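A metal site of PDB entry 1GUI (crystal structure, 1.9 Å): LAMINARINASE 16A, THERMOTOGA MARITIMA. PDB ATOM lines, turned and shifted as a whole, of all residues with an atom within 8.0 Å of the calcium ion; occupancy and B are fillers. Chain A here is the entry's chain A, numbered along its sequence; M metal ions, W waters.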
ATOM      1  N   ASN A   4       8.058  33.404   4.476  1.00  0.00           N
ATOM      2  CA  ASN A   4       7.188  32.646   5.397  1.00  0.00           C
ATOM      3  C   ASN A   4       5.795  32.397   4.794  1.00  0.00           C
ATOM      4  O   ASN A   4       4.762  32.518   5.441  1.00  0.00           O
ATOM      5  CB  ASN A   4       7.093  33.362   6.755  1.00  0.00           C
ATOM      6  CG  ASN A   4       6.462  32.489   7.844  1.00  0.00           C
ATOM      7  OD1 ASN A   4       6.666  31.269   7.918  1.00  0.00           O
ATOM      8  ND2 ASN A   4       5.706  33.130   8.734  1.00  0.00           N
ATOM      9  N   GLY A   5       5.805  32.060   3.518  1.00  0.00           N
ATOM     10  CA  GLY A   5       4.602  31.665   2.794  1.00  0.00           C
ATOM     11  C   GLY A   5       4.057  30.301   3.231  1.00  0.00           C
ATOM     12  O   GLY A   5       2.897  30.006   2.937  1.00  0.00           O
ATOM     13  N   THR A   6       4.859  29.492   3.920  1.00  0.00           N
ATOM     14  CA  THR A   6       4.423  28.196   4.461  1.00  0.00           C
ATOM     15  C   THR A   6       3.909  28.253   5.902  1.00  0.00           C
ATOM     16  O   THR A   6       3.353  27.277   6.408  1.00  0.00           O
ATOM     17  CB  THR A   6       5.598  27.173   4.461  1.00  0.00           C
ATOM     18  OG1 THR A   6       6.677  27.701   5.245  1.00  0.00           O
ATOM     19  CG2 THR A   6       6.178  26.955   3.039  1.00  0.00           C
ATOM     20  N   PHE A   7       4.168  29.359   6.595  1.00  0.00           N
ATOM     21  CA  PHE A   7       3.784  29.553   7.997  1.00  0.00           C
ATOM     22  C   PHE A   7       4.388  28.593   9.003  1.00  0.00           C
ATOM     23  O   PHE A   7       3.745  28.235   9.999  1.00  0.00           O
ATOM     24  CB  PHE A   7       2.252  29.647   8.094  1.00  0.00           C
ATOM     25  CG  PHE A   7       1.715  30.762   7.253  1.00  0.00           C
ATOM     26  CD1 PHE A   7       2.018  32.070   7.569  1.00  0.00           C
ATOM     27  CD2 PHE A   7       0.967  30.523   6.125  1.00  0.00           C
ATOM     28  CE1 PHE A   7       1.563  33.120   6.778  1.00  0.00           C
ATOM     29  CE2 PHE A   7       0.516  31.545   5.343  1.00  0.00           C
ATOM     30  CZ  PHE A   7       0.804  32.849   5.665  1.00  0.00           C
ATOM     31  N   ASP A   8       5.640  28.199   8.759  1.00  0.00           N
ATOM     32  CA  ASP A   8       6.443  27.422   9.719  1.00  0.00           C
ATOM     33  C   ASP A   8       7.009  28.331  10.827  1.00  0.00           C
ATOM     34  O   ASP A   8       7.473  27.845  11.854  1.00  0.00           O
ATOM     35  CB  ASP A   8       7.606  26.717   8.989  1.00  0.00           C
ATOM     36  CG  ASP A   8       7.137  25.591   8.036  1.00  0.00           C
ATOM     37  OD1 ASP A   8       6.005  25.073   8.192  1.00  0.00           O
ATOM     38  OD2 ASP A   8       7.853  25.159   7.113  1.00  0.00           O
ATOM     39  N   GLU A   9       7.009  29.644  10.590  1.00  0.00           N
ATOM     40  CA  GLU A   9       7.542  30.630  11.538  1.00  0.00           C
ATOM     41  C   GLU A   9       6.407  31.597  11.930  1.00  0.00           C
ATOM     42  O   GLU A   9       5.439  31.748  11.188  1.00  0.00           O
ATOM     43  CB  GLU A   9       8.717  31.410  10.908  1.00  0.00           C
ATOM     44  CG  GLU A   9       9.970  30.589  10.595  1.00  0.00           C
ATOM     45  CD  GLU A   9      10.601  29.936  11.807  1.00  0.00           C
ATOM     46  OE1 GLU A   9      10.503  30.505  12.914  1.00  0.00           O
ATOM     47  OE2 GLU A   9      11.223  28.845  11.663  1.00  0.00           O
ATOM     48  N   ARG A  43      -0.262  27.953  13.757  1.00  0.00           N
ATOM     49  CA  ARG A  43      -0.234  26.631  14.386  1.00  0.00           C
ATOM     50  C   ARG A  43      -0.350  25.521  13.350  1.00  0.00           C
ATOM     51  O   ARG A  43      -1.060  25.644  12.343  1.00  0.00           O
ATOM     52  CB  ARG A  43      -1.284  26.492  15.490  1.00  0.00           C
ATOM     53  CG  ARG A  43      -2.781  26.342  15.070  1.00  0.00           C
ATOM     54  CD  ARG A  43      -3.728  25.745  16.212  1.00  0.00           C
ATOM     55  NE  ARG A  43      -3.930  26.642  17.359  1.00  0.00           N
ATOM     56  CZ  ARG A  43      -4.873  27.624  17.463  1.00  0.00           C
ATOM     57  NH1 ARG A  43      -5.763  27.871  16.500  1.00  0.00           N
ATOM     58  NH2 ARG A  43      -4.919  28.370  18.572  1.00  0.00           N
ATOM     59  N   ASP A  44       0.366  24.422  13.588  1.00  0.00           N
ATOM     60  CA  ASP A  44       0.314  23.255  12.706  1.00  0.00           C
ATOM     61  C   ASP A  44       0.512  23.579  11.224  1.00  0.00           C
ATOM     62  O   ASP A  44      -0.103  22.967  10.382  1.00  0.00           O
ATOM     63  CB  ASP A  44      -1.020  22.515  12.876  1.00  0.00           C
ATOM     64  CG  ASP A  44      -1.237  22.027  14.289  1.00  0.00           C
ATOM     65  OD1 ASP A  44      -0.225  21.665  14.948  1.00  0.00           O
ATOM     66  OD2 ASP A  44      -2.361  21.954  14.813  1.00  0.00           O
ATOM     67  N   GLY A  45       1.385  24.543  10.924  1.00  0.00           N
ATOM     68  CA  GLY A  45       1.738  24.866   9.542  1.00  0.00           C
ATOM     69  C   GLY A  45       0.851  25.823   8.766  1.00  0.00           C
ATOM     70  O   GLY A  45       1.025  25.950   7.531  1.00  0.00           O
ATOM     71  N   TYR A  46      -0.092  26.465   9.447  1.00  0.00           N
ATOM     72  CA  TYR A  46      -0.995  27.447   8.820  1.00  0.00           C
ATOM     73  C   TYR A  46      -1.161  28.694   9.703  1.00  0.00           C
ATOM     74  O   TYR A  46      -0.909  28.647  10.903  1.00  0.00           O
ATOM     75  CB  TYR A  46      -2.364  26.815   8.500  1.00  0.00           C
ATOM     76  CG  TYR A  46      -3.122  26.297   9.698  1.00  0.00           C
ATOM     77  CD1 TYR A  46      -3.827  27.161  10.534  1.00  0.00           C
ATOM     78  CD2 TYR A  46      -3.121  24.946  10.007  1.00  0.00           C
ATOM     79  CE1 TYR A  46      -4.529  26.665  11.663  1.00  0.00           C
ATOM     80  CE2 TYR A  46      -3.807  24.429  11.116  1.00  0.00           C
ATOM     81  CZ  TYR A  46      -4.510  25.310  11.950  1.00  0.00           C
ATOM     82  OH  TYR A  46      -5.183  24.830  13.082  1.00  0.00           O
ATOM     83  N   ALA A  47      -1.517  29.801   9.067  1.00  0.00           N
ATOM     84  CA  ALA A  47      -1.901  31.073   9.712  1.00  0.00           C
ATOM     85  C   ALA A  47      -3.414  31.145  10.032  1.00  0.00           C
ATOM     86  O   ALA A  47      -4.242  30.641   9.264  1.00  0.00           O
ATOM     87  CB  ALA A  47      -1.521  32.232   8.809  1.00  0.00           C
ATOM     88  N   LYS A  80      -3.748  28.977  -0.450  1.00  0.00           N
ATOM     89  CA  LYS A  80      -4.798  28.173   0.156  1.00  0.00           C
ATOM     90  C   LYS A  80      -5.490  28.996   1.249  1.00  0.00           C
ATOM     91  O   LYS A  80      -4.853  29.748   1.964  1.00  0.00           O
ATOM     92  CB  LYS A  80      -4.249  26.903   0.778  1.00  0.00           C
ATOM     93  CG  LYS A  80      -3.598  25.939  -0.203  1.00  0.00           C
ATOM     94  CD  LYS A  80      -3.101  24.656   0.516  1.00  0.00           C
ATOM     95  CE  LYS A  80      -2.542  23.686  -0.475  1.00  0.00           C
ATOM     96  NZ  LYS A  80      -1.540  22.772   0.138  1.00  0.00           N
ATOM     97  N   TRP A 114     -10.607  23.704   3.320  1.00  0.00           N
ATOM     98  CA  TRP A 114      -9.455  24.231   2.608  1.00  0.00           C
ATOM     99  C   TRP A 114      -9.655  24.126   1.082  1.00  0.00           C
ATOM    100  O   TRP A 114     -10.016  23.057   0.585  1.00  0.00           O
ATOM    101  CB  TRP A 114      -8.179  23.457   2.958  1.00  0.00           C
ATOM    102  CG  TRP A 114      -7.583  23.753   4.329  1.00  0.00           C
ATOM    103  CD1 TRP A 114      -7.610  22.953   5.437  1.00  0.00           C
ATOM    104  CD2 TRP A 114      -6.852  24.918   4.697  1.00  0.00           C
ATOM    105  NE1 TRP A 114      -6.950  23.561   6.482  1.00  0.00           N
ATOM    106  CE2 TRP A 114      -6.494  24.781   6.054  1.00  0.00           C
ATOM    107  CE3 TRP A 114      -6.493  26.099   4.021  1.00  0.00           C
ATOM    108  CZ2 TRP A 114      -5.744  25.759   6.728  1.00  0.00           C
ATOM    109  CZ3 TRP A 114      -5.771  27.078   4.691  1.00  0.00           C
ATOM    110  CH2 TRP A 114      -5.393  26.893   6.037  1.00  0.00           C
ATOM    111  N   PHE A 147      -4.926  30.759   6.300  1.00  0.00           N
ATOM    112  CA  PHE A 147      -4.098  30.802   5.079  1.00  0.00           C
ATOM    113  C   PHE A 147      -2.958  29.774   5.116  1.00  0.00           C
ATOM    114  O   PHE A 147      -2.429  29.434   6.188  1.00  0.00           O
ATOM    115  CB  PHE A 147      -3.465  32.191   4.856  1.00  0.00           C
ATOM    116  CG  PHE A 147      -4.461  33.290   4.574  1.00  0.00           C
ATOM    117  CD1 PHE A 147      -4.882  33.502   3.281  1.00  0.00           C
ATOM    118  CD2 PHE A 147      -4.938  34.128   5.591  1.00  0.00           C
ATOM    119  CE1 PHE A 147      -5.812  34.516   2.966  1.00  0.00           C
ATOM    120  CE2 PHE A 147      -5.855  35.154   5.285  1.00  0.00           C
ATOM    121  CZ  PHE A 147      -6.296  35.336   3.971  1.00  0.00           C
ATOM    122  N   ASP A 148      -2.568  29.290   3.927  1.00  0.00           N
ATOM    123  CA  ASP A 148      -1.375  28.436   3.792  1.00  0.00           C
ATOM    124  C   ASP A 148      -0.809  28.513   2.341  1.00  0.00           C
ATOM    125  O   ASP A 148      -1.493  28.903   1.438  1.00  0.00           O
ATOM    126  CB  ASP A 148      -1.713  27.001   4.162  1.00  0.00           C
ATOM    127  CG  ASP A 148      -0.482  26.182   4.595  1.00  0.00           C
ATOM    128  OD1 ASP A 148       0.644  26.726   4.705  1.00  0.00           O
ATOM    129  OD2 ASP A 148      -0.557  24.963   4.845  1.00  0.00           O
ATOM    130  N   ASP A 149       0.454  28.139   2.167  1.00  0.00           N
ATOM    131  CA  ASP A 149       1.094  27.960   0.870  1.00  0.00           C
ATOM    132  C   ASP A 149       0.894  29.141  -0.077  1.00  0.00           C
ATOM    133  O   ASP A 149       0.439  28.991  -1.204  1.00  0.00           O
ATOM    134  CB  ASP A 149       0.660  26.614   0.243  1.00  0.00           C
ATOM    135  CG  ASP A 149       1.088  25.418   1.065  1.00  0.00           C
ATOM    136  OD1 ASP A 149       2.283  25.330   1.447  1.00  0.00           O
ATOM    137  OD2 ASP A 149       0.314  24.495   1.384  1.00  0.00           O
ATOM    138  N   VAL A 150       1.213  30.347   0.417  1.00  0.00           N
ATOM    139  CA  VAL A 150       1.204  31.574  -0.410  1.00  0.00           C
ATOM    140  C   VAL A 150       2.498  31.695  -1.210  1.00  0.00           C
ATOM    141  O   VAL A 150       3.615  31.695  -0.623  1.00  0.00           O
ATOM    142  CB  VAL A 150       1.055  32.842   0.464  1.00  0.00           C
ATOM    143  CG1 VAL A 150       0.943  34.099  -0.424  1.00  0.00           C
ATOM    144  CG2 VAL A 150      -0.159  32.736   1.392  1.00  0.00           C
HETATM  145 CA    CA M   1       2.279  25.366   5.812  1.00  0.00          CA
HETATM  146  O   HOH W   1       3.134  25.105   4.051  1.00  0.00           O
HETATM  147  O   HOH W   2       1.195  23.317   5.879  1.00  0.00           O
HETATM  148  O   HOH W   3       4.116  24.226   6.594  1.00  0.00           O
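Water W1 binds the calcium ion (2.0 Å).
The calcium ion is bound by O of Gly 45 (2.2 Å).
The backbone carbonyl oxygen (O) of Thr 6 is bound to the calcium ion (2.3 Å).
Water W3 binds the calcium ion, at 2.3 Å.
Water W2 is bound to the calcium ion.
OD1 of Asp 148 is bound to the calcium ion, 2.4 Å away.
Slightly farther from the calcium ion lies OD2 of Asp 148 (3.0 Å).
OD2 of Asp 8 lies within hydrogen-bond range of OG1 of Thr 6 (3.4 Å).
The backbone carbonyl oxygen (O) of Asp 148 sits at hydrogen-bond distance from the backbone NH (N) of Lys 80 (2.9 Å).
Within 4 Å of the calcium ion: Thr 6, Gly 45 and Asp 148.
Along chain A the residues within 4 Å of the calcium ion span positions 6 to 148.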
